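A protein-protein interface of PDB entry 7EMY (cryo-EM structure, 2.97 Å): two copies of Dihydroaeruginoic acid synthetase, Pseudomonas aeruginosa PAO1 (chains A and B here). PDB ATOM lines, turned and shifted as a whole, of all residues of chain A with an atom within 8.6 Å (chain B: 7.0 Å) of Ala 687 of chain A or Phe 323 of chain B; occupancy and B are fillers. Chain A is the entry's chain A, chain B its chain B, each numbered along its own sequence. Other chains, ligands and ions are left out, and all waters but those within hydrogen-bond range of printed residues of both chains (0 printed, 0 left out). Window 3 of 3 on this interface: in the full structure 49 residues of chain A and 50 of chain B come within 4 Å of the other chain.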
ATOM      1  N   ALA A 553     -28.162  33.335  22.465  1.00  0.00           N
ATOM      2  CA  ALA A 553     -27.461  32.756  21.383  1.00  0.00           C
ATOM      3  C   ALA A 553     -27.830  33.420  20.084  1.00  0.00           C
ATOM      4  O   ALA A 553     -28.981  33.289  19.658  1.00  0.00           O
ATOM      5  CB  ALA A 553     -27.550  31.339  21.313  1.00  0.00           C
ATOM      6  N   ARG A 554     -26.964  34.113  19.429  1.00  0.00           N
ATOM      7  CA  ARG A 554     -27.148  34.915  18.285  1.00  0.00           C
ATOM      8  C   ARG A 554     -25.878  35.162  17.525  1.00  0.00           C
ATOM      9  O   ARG A 554     -24.792  35.027  18.093  1.00  0.00           O
ATOM     10  CB  ARG A 554     -27.818  36.175  18.607  1.00  0.00           C
ATOM     11  CG  ARG A 554     -27.116  37.147  19.391  1.00  0.00           C
ATOM     12  CD  ARG A 554     -27.753  38.299  19.935  1.00  0.00           C
ATOM     13  NE  ARG A 554     -27.045  39.161  20.752  1.00  0.00           N
ATOM     14  CZ  ARG A 554     -26.664  38.989  21.976  1.00  0.00           C
ATOM     15  NH1 ARG A 554     -26.997  37.964  22.557  1.00  0.00           N
ATOM     16  NH2 ARG A 554     -25.996  39.832  22.574  1.00  0.00           N
ATOM     17  N   THR A 555     -25.932  35.556  16.300  1.00  0.00           N
ATOM     18  CA  THR A 555     -24.860  36.024  15.517  1.00  0.00           C
ATOM     19  C   THR A 555     -24.238  37.237  16.156  1.00  0.00           C
ATOM     20  O   THR A 555     -24.965  38.099  16.654  1.00  0.00           O
ATOM     21  CB  THR A 555     -25.132  36.281  14.073  1.00  0.00           C
ATOM     22  OG1 THR A 555     -23.985  36.596  13.337  1.00  0.00           O
ATOM     23  CG2 THR A 555     -26.152  37.237  13.909  1.00  0.00           C
ATOM     24  N   LEU A 556     -22.919  37.366  16.135  1.00  0.00           N
ATOM     25  CA  LEU A 556     -22.217  38.384  16.914  1.00  0.00           C
ATOM     26  C   LEU A 556     -22.555  39.806  16.464  1.00  0.00           C
ATOM     27  O   LEU A 556     -22.519  40.738  17.254  1.00  0.00           O
ATOM     28  CB  LEU A 556     -20.726  38.068  16.790  1.00  0.00           C
ATOM     29  CG  LEU A 556     -19.763  38.884  17.632  1.00  0.00           C
ATOM     30  CD1 LEU A 556     -20.052  38.732  19.113  1.00  0.00           C
ATOM     31  CD2 LEU A 556     -18.350  38.394  17.371  1.00  0.00           C
ATOM     32  N   HIS A 557     -22.941  39.977  15.197  1.00  0.00           N
ATOM     33  CA  HIS A 557     -23.278  41.201  14.582  1.00  0.00           C
ATOM     34  C   HIS A 557     -24.696  41.653  14.818  1.00  0.00           C
ATOM     35  O   HIS A 557     -25.040  42.807  14.547  1.00  0.00           O
ATOM     36  CB  HIS A 557     -22.968  41.230  13.150  1.00  0.00           C
ATOM     37  CG  HIS A 557     -23.711  40.314  12.294  1.00  0.00           C
ATOM     38  ND1 HIS A 557     -23.208  39.281  11.614  1.00  0.00           N
ATOM     39  CD2 HIS A 557     -24.986  40.192  12.018  1.00  0.00           C
ATOM     40  CE1 HIS A 557     -24.084  38.645  11.020  1.00  0.00           C
ATOM     41  NE2 HIS A 557     -25.238  39.154  11.225  1.00  0.00           N
ATOM     42  N   PRO A 603     -20.678  32.773   3.581  1.00  0.00           N
ATOM     43  CA  PRO A 603     -20.739  32.515   5.027  1.00  0.00           C
ATOM     44  C   PRO A 603     -19.622  31.639   5.570  1.00  0.00           C
ATOM     45  O   PRO A 603     -19.345  30.555   5.046  1.00  0.00           O
ATOM     46  CB  PRO A 603     -22.102  31.835   5.193  1.00  0.00           C
ATOM     47  CG  PRO A 603     -22.931  32.432   4.122  1.00  0.00           C
ATOM     48  CD  PRO A 603     -22.005  32.637   2.953  1.00  0.00           C
ATOM     49  N   GLY A 628     -21.575  37.091   6.389  1.00  0.00           N
ATOM     50  CA  GLY A 628     -21.463  35.822   6.887  1.00  0.00           C
ATOM     51  C   GLY A 628     -20.135  35.253   7.141  1.00  0.00           C
ATOM     52  O   GLY A 628     -19.989  34.113   7.600  1.00  0.00           O
ATOM     53  N   VAL A 684     -26.161  38.776   6.379  1.00  0.00           N
ATOM     54  CA  VAL A 684     -26.343  37.428   5.981  1.00  0.00           C
ATOM     55  C   VAL A 684     -26.786  36.612   7.166  1.00  0.00           C
ATOM     56  O   VAL A 684     -26.102  36.683   8.206  1.00  0.00           O
ATOM     57  CB  VAL A 684     -25.221  36.806   5.194  1.00  0.00           C
ATOM     58  CG1 VAL A 684     -25.434  35.444   4.884  1.00  0.00           C
ATOM     59  CG2 VAL A 684     -24.840  37.564   4.058  1.00  0.00           C
ATOM     60  N   PRO A 685     -27.863  35.828   7.115  1.00  0.00           N
ATOM     61  CA  PRO A 685     -28.288  35.091   8.314  1.00  0.00           C
ATOM     62  C   PRO A 685     -27.292  34.009   8.696  1.00  0.00           C
ATOM     63  O   PRO A 685     -27.169  32.987   8.017  1.00  0.00           O
ATOM     64  CB  PRO A 685     -29.640  34.498   7.902  1.00  0.00           C
ATOM     65  CG  PRO A 685     -29.575  34.403   6.423  1.00  0.00           C
ATOM     66  CD  PRO A 685     -28.755  35.574   5.970  1.00  0.00           C
ATOM     67  N   LEU A 686     -26.578  34.175   9.755  1.00  0.00           N
ATOM     68  CA  LEU A 686     -25.635  33.311  10.348  1.00  0.00           C
ATOM     69  C   LEU A 686     -26.187  32.566  11.528  1.00  0.00           C
ATOM     70  O   LEU A 686     -26.772  33.202  12.410  1.00  0.00           O
ATOM     71  CB  LEU A 686     -24.320  33.918  10.604  1.00  0.00           C
ATOM     72  CG  LEU A 686     -23.257  34.172   9.623  1.00  0.00           C
ATOM     73  CD1 LEU A 686     -22.077  34.694  10.196  1.00  0.00           C
ATOM     74  CD2 LEU A 686     -23.016  33.043   8.805  1.00  0.00           C
ATOM     75  N   ALA A 687     -26.032  31.297  11.632  1.00  0.00           N
ATOM     76  CA  ALA A 687     -26.208  30.516  12.783  1.00  0.00           C
ATOM     77  C   ALA A 687     -25.238  30.948  13.855  1.00  0.00           C
ATOM     78  O   ALA A 687     -24.071  31.183  13.528  1.00  0.00           O
ATOM     79  CB  ALA A 687     -26.199  29.113  12.570  1.00  0.00           C
ATOM     80  N   PRO A 688     -25.638  31.059  15.125  1.00  0.00           N
ATOM     81  CA  PRO A 688     -24.709  31.506  16.149  1.00  0.00           C
ATOM     82  C   PRO A 688     -23.444  30.714  16.272  1.00  0.00           C
ATOM     83  O   PRO A 688     -22.404  31.221  16.711  1.00  0.00           O
ATOM     84  CB  PRO A 688     -25.552  31.556  17.350  1.00  0.00           C
ATOM     85  CG  PRO A 688     -26.878  31.501  16.942  1.00  0.00           C
ATOM     86  CD  PRO A 688     -26.895  30.806  15.739  1.00  0.00           C
ATOM     87  N   GLN A 689     -23.453  29.464  15.948  1.00  0.00           N
ATOM     88  CA  GLN A 689     -22.394  28.537  16.019  1.00  0.00           C
ATOM     89  C   GLN A 689     -21.295  28.790  15.023  1.00  0.00           C
ATOM     90  O   GLN A 689     -20.200  28.229  15.137  1.00  0.00           O
ATOM     91  CB  GLN A 689     -22.851  27.142  16.071  1.00  0.00           C
ATOM     92  CG  GLN A 689     -23.852  26.744  17.016  1.00  0.00           C
ATOM     93  CD  GLN A 689     -25.247  27.131  16.739  1.00  0.00           C
ATOM     94  OE1 GLN A 689     -25.605  27.239  15.566  1.00  0.00           O
ATOM     95  NE2 GLN A 689     -25.996  27.363  17.686  1.00  0.00           N
ATOM     96  N   ALA A 690     -21.512  29.567  14.018  1.00  0.00           N
ATOM     97  CA  ALA A 690     -20.634  29.886  12.965  1.00  0.00           C
ATOM     98  C   ALA A 690     -19.415  30.626  13.455  1.00  0.00           C
ATOM     99  O   ALA A 690     -19.481  31.329  14.467  1.00  0.00           O
ATOM    100  CB  ALA A 690     -21.235  30.528  11.848  1.00  0.00           C
ATOM    101  N   SER A 691     -18.309  30.543  12.797  1.00  0.00           N
ATOM    102  CA  SER A 691     -17.094  31.207  13.049  1.00  0.00           C
ATOM    103  C   SER A 691     -17.270  32.701  13.003  1.00  0.00           C
ATOM    104  O   SER A 691     -17.847  33.200  12.032  1.00  0.00           O
ATOM    105  CB  SER A 691     -15.970  30.699  12.256  1.00  0.00           C
ATOM    106  OG  SER A 691     -15.780  29.365  12.316  1.00  0.00           O
ATOM    107  N   ALA A 692     -16.814  33.454  13.947  1.00  0.00           N
ATOM    108  CA  ALA A 692     -16.841  34.859  14.079  1.00  0.00           C
ATOM    109  C   ALA A 692     -15.563  35.547  13.681  1.00  0.00           C
ATOM    110  O   ALA A 692     -15.519  36.407  12.796  1.00  0.00           O
ATOM    111  CB  ALA A 692     -17.318  35.312  15.343  1.00  0.00           C
ATOM    112  N   SER A 710     -16.370  31.188  17.485  1.00  0.00           N
ATOM    113  CA  SER A 710     -17.702  31.204  17.040  1.00  0.00           C
ATOM    114  C   SER A 710     -18.422  32.455  17.472  1.00  0.00           C
ATOM    115  O   SER A 710     -18.062  33.060  18.486  1.00  0.00           O
ATOM    116  CB  SER A 710     -18.469  30.014  17.407  1.00  0.00           C
ATOM    117  OG  SER A 710     -18.537  29.858  18.747  1.00  0.00           O
ATOM    118  N   HIS A 711     -19.441  32.873  16.796  1.00  0.00           N
ATOM    119  CA  HIS A 711     -20.352  33.876  17.186  1.00  0.00           C
ATOM    120  C   HIS A 711     -20.960  33.567  18.524  1.00  0.00           C
ATOM    121  O   HIS A 711     -21.129  34.428  19.394  1.00  0.00           O
ATOM    122  CB  HIS A 711     -21.314  34.245  16.140  1.00  0.00           C
ATOM    123  CG  HIS A 711     -20.855  34.687  14.832  1.00  0.00           C
ATOM    124  ND1 HIS A 711     -20.560  36.004  14.556  1.00  0.00           N
ATOM    125  CD2 HIS A 711     -20.560  34.068  13.717  1.00  0.00           C
ATOM    126  CE1 HIS A 711     -20.133  36.040  13.352  1.00  0.00           C
ATOM    127  NE2 HIS A 711     -20.127  34.914  12.851  1.00  0.00           N
ATOM    128  N   ALA A 712     -21.328  32.349  18.753  1.00  0.00           N
ATOM    129  CA  ALA A 712     -21.920  31.845  19.928  1.00  0.00           C
ATOM    130  C   ALA A 712     -21.070  32.101  21.143  1.00  0.00           C
ATOM    131  O   ALA A 712     -21.512  32.635  22.161  1.00  0.00           O
ATOM    132  CB  ALA A 712     -22.356  30.492  19.848  1.00  0.00           C
ATOM    133  N   ARG A 901     -14.105  27.392  18.622  1.00  0.00           N
ATOM    134  CA  ARG A 901     -14.308  26.263  17.802  1.00  0.00           C
ATOM    135  C   ARG A 901     -13.073  25.411  17.708  1.00  0.00           C
ATOM    136  O   ARG A 901     -13.127  24.217  17.392  1.00  0.00           O
ATOM    137  CB  ARG A 901     -14.932  26.592  16.515  1.00  0.00           C
ATOM    138  CG  ARG A 901     -16.014  27.529  16.407  1.00  0.00           C
ATOM    139  CD  ARG A 901     -16.674  27.668  15.142  1.00  0.00           C
ATOM    140  NE  ARG A 901     -15.928  27.449  13.996  1.00  0.00           N
ATOM    141  CZ  ARG A 901     -16.004  26.542  13.074  1.00  0.00           C
ATOM    142  NH1 ARG A 901     -16.934  25.745  13.103  1.00  0.00           N
ATOM    143  NH2 ARG A 901     -15.186  26.470  12.156  1.00  0.00           N
ATOM    144  N   ARG B 320     -38.117  22.357  10.381  1.00  0.00           N
ATOM    145  CA  ARG B 320     -36.708  22.254   9.988  1.00  0.00           C
ATOM    146  C   ARG B 320     -35.817  23.005  10.960  1.00  0.00           C
ATOM    147  O   ARG B 320     -36.041  24.177  11.238  1.00  0.00           O
ATOM    148  CB  ARG B 320     -36.483  22.787   8.567  1.00  0.00           C
ATOM    149  CG  ARG B 320     -34.985  22.782   8.223  1.00  0.00           C
ATOM    150  CD  ARG B 320     -34.685  22.863   6.735  1.00  0.00           C
ATOM    151  NE  ARG B 320     -34.958  21.572   6.112  1.00  0.00           N
ATOM    152  CZ  ARG B 320     -34.446  21.068   5.021  1.00  0.00           C
ATOM    153  NH1 ARG B 320     -33.584  21.710   4.289  1.00  0.00           N
ATOM    154  NH2 ARG B 320     -34.798  19.883   4.664  1.00  0.00           N
ATOM    155  N   LEU B 321     -34.733  22.370  11.358  1.00  0.00           N
ATOM    156  CA  LEU B 321     -33.593  22.867  12.020  1.00  0.00           C
ATOM    157  C   LEU B 321     -32.414  22.917  11.091  1.00  0.00           C
ATOM    158  O   LEU B 321     -31.846  21.859  10.805  1.00  0.00           O
ATOM    159  CB  LEU B 321     -33.350  22.224  13.315  1.00  0.00           C
ATOM    160  CG  LEU B 321     -34.384  22.106  14.351  1.00  0.00           C
ATOM    161  CD1 LEU B 321     -34.053  21.247  15.416  1.00  0.00           C
ATOM    162  CD2 LEU B 321     -34.835  23.376  14.786  1.00  0.00           C
ATOM    163  N   ALA B 322     -32.011  24.033  10.588  1.00  0.00           N
ATOM    164  CA  ALA B 322     -31.087  24.287   9.556  1.00  0.00           C
ATOM    165  C   ALA B 322     -29.790  24.861  10.046  1.00  0.00           C
ATOM    166  O   ALA B 322     -29.820  25.808  10.837  1.00  0.00           O
ATOM    167  CB  ALA B 322     -31.607  25.030   8.457  1.00  0.00           C
ATOM    168  N   PHE B 323     -28.663  24.387   9.630  1.00  0.00           N
ATOM    169  CA  PHE B 323     -27.349  24.861   9.843  1.00  0.00           C
ATOM    170  C   PHE B 323     -26.523  24.788   8.587  1.00  0.00           C
ATOM    171  O   PHE B 323     -26.151  23.677   8.197  1.00  0.00           O
ATOM    172  CB  PHE B 323     -26.631  24.317  10.996  1.00  0.00           C
ATOM    173  CG  PHE B 323     -25.350  24.882  11.391  1.00  0.00           C
ATOM    174  CD1 PHE B 323     -25.239  25.975  12.167  1.00  0.00           C
ATOM    175  CD2 PHE B 323     -24.163  24.419  10.955  1.00  0.00           C
ATOM    176  CE1 PHE B 323     -24.098  26.530  12.475  1.00  0.00           C
ATOM    177  CE2 PHE B 323     -23.021  24.967  11.259  1.00  0.00           C
ATOM    178  CZ  PHE B 323     -22.988  26.025  12.019  1.00  0.00           C
ATOM    179  N   GLN B 324     -26.216  25.849   7.928  1.00  0.00           N
ATOM    180  CA  GLN B 324     -25.424  25.989   6.765  1.00  0.00           C
ATOM    181  C   GLN B 324     -23.966  25.892   7.116  1.00  0.00           C
ATOM    182  O   GLN B 324     -23.358  26.916   7.436  1.00  0.00           O
ATOM    183  CB  GLN B 324     -25.697  27.140   5.902  1.00  0.00           C
ATOM    184  CG  GLN B 324     -24.811  27.452   4.813  1.00  0.00           C
ATOM    185  CD  GLN B 324     -24.666  26.444   3.751  1.00  0.00           C
ATOM    186  OE1 GLN B 324     -25.298  25.392   3.850  1.00  0.00           O
ATOM    187  NE2 GLN B 324     -23.926  26.686   2.797  1.00  0.00           N
ATOM    188  N   LEU B 325     -23.349  24.759   7.111  1.00  0.00           N
ATOM    189  CA  LEU B 325     -21.964  24.550   7.249  1.00  0.00           C
ATOM    190  C   LEU B 325     -21.216  25.388   6.252  1.00  0.00           C
ATOM    191  O   LEU B 325     -21.517  25.302   5.058  1.00  0.00           O
ATOM    192  CB  LEU B 325     -21.550  23.140   7.305  1.00  0.00           C
ATOM    193  CG  LEU B 325     -21.620  22.278   8.496  1.00  0.00           C
ATOM    194  CD1 LEU B 325     -21.462  20.904   8.240  1.00  0.00           C
ATOM    195  CD2 LEU B 325     -20.764  22.724   9.526  1.00  0.00           C
ATOM    196  N   SER B 326     -20.252  26.182   6.700  1.00  0.00           N
ATOM    197  CA  SER B 326     -19.562  27.090   5.802  1.00  0.00           C
ATOM    198  C   SER B 326     -18.722  26.313   4.796  1.00  0.00           C
ATOM    199  O   SER B 326     -18.456  25.119   4.952  1.00  0.00           O
ATOM    200  CB  SER B 326     -18.677  28.047   6.594  1.00  0.00           C
ATOM    201  OG  SER B 326     -17.675  27.343   7.303  1.00  0.00           O
ATOM    202  N   GLU B 329     -15.678  25.020   6.561  1.00  0.00           N
ATOM    203  CA  GLU B 329     -16.106  23.936   7.359  1.00  0.00           C
ATOM    204  C   GLU B 329     -16.253  22.674   6.551  1.00  0.00           C
ATOM    205  O   GLU B 329     -15.792  21.586   6.918  1.00  0.00           O
ATOM    206  CB  GLU B 329     -17.242  24.255   8.236  1.00  0.00           C
ATOM    207  CG  GLU B 329     -17.136  25.095   9.396  1.00  0.00           C
ATOM    208  CD  GLU B 329     -18.341  25.593  10.082  1.00  0.00           C
ATOM    209  OE1 GLU B 329     -19.385  25.634   9.397  1.00  0.00           O
ATOM    210  OE2 GLU B 329     -18.303  25.929  11.284  1.00  0.00           O
ATOM    211  N   ILE B 490     -22.354  22.928   3.156  1.00  0.00           N
ATOM    212  CA  ILE B 490     -23.209  21.878   3.554  1.00  0.00           C
ATOM    213  C   ILE B 490     -24.367  22.375   4.376  1.00  0.00           C
ATOM    214  O   ILE B 490     -24.122  23.058   5.377  1.00  0.00           O
ATOM    215  CB  ILE B 490     -22.536  20.671   4.130  1.00  0.00           C
ATOM    216  CG1 ILE B 490     -21.400  20.164   3.352  1.00  0.00           C
ATOM    217  CG2 ILE B 490     -23.438  19.649   4.466  1.00  0.00           C
ATOM    218  CD1 ILE B 490     -20.553  19.230   3.875  1.00  0.00           C
ATOM    219  N   LEU B 491     -25.586  22.093   4.062  1.00  0.00           N
ATOM    220  CA  LEU B 491     -26.794  22.413   4.723  1.00  0.00           C
ATOM    221  C   LEU B 491     -27.245  21.299   5.628  1.00  0.00           C
ATOM    222  O   LEU B 491     -27.850  20.343   5.134  1.00  0.00           O
ATOM    223  CB  LEU B 491     -27.899  22.893   3.891  1.00  0.00           C
ATOM    224  CG  LEU B 491     -29.263  23.100   4.404  1.00  0.00           C
ATOM    225  CD1 LEU B 491     -29.265  23.956   5.527  1.00  0.00           C
ATOM    226  CD2 LEU B 491     -30.214  23.473   3.435  1.00  0.00           C
ATOM    227  N   LEU B 492     -27.007  21.323   6.895  1.00  0.00           N
ATOM    228  CA  LEU B 492     -27.470  20.437   7.888  1.00  0.00           C
ATOM    229  C   LEU B 492     -28.924  20.674   8.181  1.00  0.00           C
ATOM    230  O   LEU B 492     -29.255  21.755   8.680  1.00  0.00           O
ATOM    231  CB  LEU B 492     -26.604  20.384   9.067  1.00  0.00           C
ATOM    232  CG  LEU B 492     -25.147  20.230   8.989  1.00  0.00           C
ATOM    233  CD1 LEU B 492     -24.468  20.437  10.203  1.00  0.00           C
ATOM    234  CD2 LEU B 492     -24.798  19.015   8.362  1.00  0.00           C
ATOM    235  N   ALA B 493     -29.815  19.781   7.927  1.00  0.00           N
ATOM    236  CA  ALA B 493     -31.217  19.826   8.062  1.00  0.00           C
ATOM    237  C   ALA B 493     -31.770  18.756   8.957  1.00  0.00           C
ATOM    238  O   ALA B 493     -31.538  17.577   8.676  1.00  0.00           O
ATOM    239  CB  ALA B 493     -31.918  19.902   6.826  1.00  0.00           C
ATOM    240  N   TRP B 494     -32.479  19.060   9.991  1.00  0.00           N
ATOM    241  CA  TRP B 494     -33.217  18.254  10.888  1.00  0.00           C
ATOM    242  C   TRP B 494     -34.692  18.504  10.743  1.00  0.00           C
ATOM    243  O   TRP B 494     -35.201  19.416  11.405  1.00  0.00           O
ATOM    244  CB  TRP B 494     -32.708  18.261  12.262  1.00  0.00           C
ATOM    245  CG  TRP B 494     -31.469  17.596  12.606  1.00  0.00           C
ATOM    246  CD1 TRP B 494     -30.454  17.328  11.804  1.00  0.00           C
ATOM    247  CD2 TRP B 494     -31.069  17.033  13.857  1.00  0.00           C
ATOM    248  NE1 TRP B 494     -29.506  16.692  12.396  1.00  0.00           N
ATOM    249  CE2 TRP B 494     -29.795  16.464  13.670  1.00  0.00           C
ATOM    250  CE3 TRP B 494     -31.594  16.929  15.106  1.00  0.00           C
ATOM    251  CZ2 TRP B 494     -29.173  15.859  14.709  1.00  0.00           C
ATOM    252  CZ3 TRP B 494     -30.946  16.331  16.066  1.00  0.00           C
ATOM    253  CH2 TRP B 494     -29.748  15.804  15.862  1.00  0.00           C
ATOM    254  N   PHE B 510     -29.897  19.324  17.798  1.00  0.00           N
ATOM    255  CA  PHE B 510     -29.363  19.854  16.606  1.00  0.00           C
ATOM    256  C   PHE B 510     -28.188  20.756  16.866  1.00  0.00           C
ATOM    257  O   PHE B 510     -27.199  20.779  16.128  1.00  0.00           O
ATOM    258  CB  PHE B 510     -30.303  20.469  15.667  1.00  0.00           C
ATOM    259  CG  PHE B 510     -29.828  20.994  14.398  1.00  0.00           C
ATOM    260  CD1 PHE B 510     -29.431  20.196  13.388  1.00  0.00           C
ATOM    261  CD2 PHE B 510     -29.679  22.304  14.130  1.00  0.00           C
ATOM    262  CE1 PHE B 510     -28.948  20.643  12.262  1.00  0.00           C
ATOM    263  CE2 PHE B 510     -29.198  22.760  13.008  1.00  0.00           C
ATOM    264  CZ  PHE B 510     -28.831  21.929  12.071  1.00  0.00           C
ATOM    265  N   VAL B 514     -24.484  20.122  15.542  1.00  0.00           N
ATOM    266  CA  VAL B 514     -23.715  21.162  14.869  1.00  0.00           C
ATOM    267  C   VAL B 514     -22.395  21.393  15.587  1.00  0.00           C
ATOM    268  O   VAL B 514     -21.348  21.571  14.956  1.00  0.00           O
ATOM    269  CB  VAL B 514     -24.539  22.457  14.786  1.00  0.00           C
ATOM    270  CG1 VAL B 514     -23.647  23.624  14.433  1.00  0.00           C
ATOM    271  CG2 VAL B 514     -25.652  22.301  13.773  1.00  0.00           C
ATOM    272  N   GLY B 515     -22.433  21.434  16.918  1.00  0.00           N
ATOM    273  CA  GLY B 515     -21.207  21.610  17.675  1.00  0.00           C
ATOM    274  C   GLY B 515     -20.227  20.484  17.434  1.00  0.00           C
ATOM    275  O   GLY B 515     -19.029  20.713  17.273  1.00  0.00           O
ATOM    276  N   LEU B 517     -19.979  18.549  14.714  1.00  0.00           N
ATOM    277  CA  LEU B 517     -19.550  18.710  13.378  1.00  0.00           C
ATOM    278  C   LEU B 517     -18.504  19.785  13.244  1.00  0.00           C
ATOM    279  O   LEU B 517     -17.461  19.622  12.602  1.00  0.00           O
ATOM    280  CB  LEU B 517     -20.642  18.773  12.405  1.00  0.00           C
ATOM    281  CG  LEU B 517     -21.446  17.595  12.058  1.00  0.00           C
ATOM    282  CD1 LEU B 517     -22.639  17.868  11.381  1.00  0.00           C
ATOM    283  CD2 LEU B 517     -20.673  16.605  11.409  1.00  0.00           C
ATOM    284  N   GLN B 518     -18.721  20.920  13.818  1.00  0.00           N
ATOM    285  CA  GLN B 518     -17.842  22.020  13.900  1.00  0.00           C
ATOM    286  C   GLN B 518     -16.542  21.662  14.561  1.00  0.00           C
ATOM    287  O   GLN B 518     -15.446  22.019  14.109  1.00  0.00           O
ATOM    288  CB  GLN B 518     -18.475  23.238  14.412  1.00  0.00           C
ATOM    289  CG  GLN B 518     -19.488  23.956  13.707  1.00  0.00           C
ATOM    290  CD  GLN B 518     -19.967  25.248  14.209  1.00  0.00           C
ATOM    291  OE1 GLN B 518     -20.214  25.368  15.408  1.00  0.00           O
ATOM    292  NE2 GLN B 518     -20.048  26.184  13.417  1.00  0.00           N
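Ala 687 of chain A touches one residue of chain B. Of the printed residues of chain B, Gln 689 of chain A touches Phe 323 (3.5 Å), Val 514 (3.96 Å) and Gln 518 (2.7 Å). Of the printed residues of chain A, Ser 326 of chain B touches Pro 603 (3.0 Å). Printed residues of chain B within 4 Å of Arg 901 of chain A: Glu 329 and Gln 518. Of the printed residues of chain A, Val 514 of chain B touches Gln 689. Of the printed residues of chain A, Glu 329 of chain B touches Arg 901 (2.3 Å).
The side-chain amide nitrogen (NE2) of Gln 518 of chain B lies within hydrogen-bond range of the backbone carbonyl oxygen (O) of Gln 689 of chain A, 2.7 Å away. NH2 of Arg 901 of chain A is in salt-bridge range of OE2 of Glu 329 of chain B (3.3 Å). The side-chain amide nitrogen of Gln 518 of chain B lies close to the guanidinium group of Arg 901 of chain A.
Of the 20 printed residues of chain A, 5 touch a printed residue of chain B. Hydrophobic or aromatic side chains of chain A that line the printed part of chain B: Ala 687. Among the printed residues, 8 pairs touch across the chains. Among the printed residues, Asp or Glu carboxylates within 4 Å of a Lys or Arg side-chain nitrogen of the other chain: Arg 901 of chain A with Glu 329 of chain B.
No position is printed for both chains. Of the 8 pairs that touch across the chains among the printed residues, none has its exchanged pair printed and touching as well.
CB of Ser 326 of chain B touches O of Pro 603 of chain A, at 3.0 Å. CB of Ala 687 of chain A touches CD1 of Phe 323 of chain B, at 3.3 Å. Gln 689 of chain A touches Phe 323 of chain B. CG1 of Val 514 of chain B touches CB of Gln 689 of chain A, at 3.96 Å. Ala 690 of chain A touches Gln 518 of chain B (N to NE2, 3.7 Å).
N of Ser 326 of chain B lies within hydrogen-bond range of OE1 of Glu 329 of chain B (2.9 Å). The side-chain carboxylate (OE2) of Glu 329 of chain B is in hydrogen-bond range of the side-chain amide nitrogen (NE2) of Gln 518 of chain B, at 2.8 Å. The backbone carbonyl oxygen of Phe 323 of chain B is in hydrogen-bond range of the backbone NH of Leu 492 of chain B (2.8 Å). OG of Ser 691 of chain A lies within hydrogen-bond range of NE of Arg 901 of chain A. The backbone NH (N) of His 711 of chain A sits at hydrogen-bond distance from the backbone carbonyl oxygen (O) of Ala 690 of chain A (2.8 Å).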
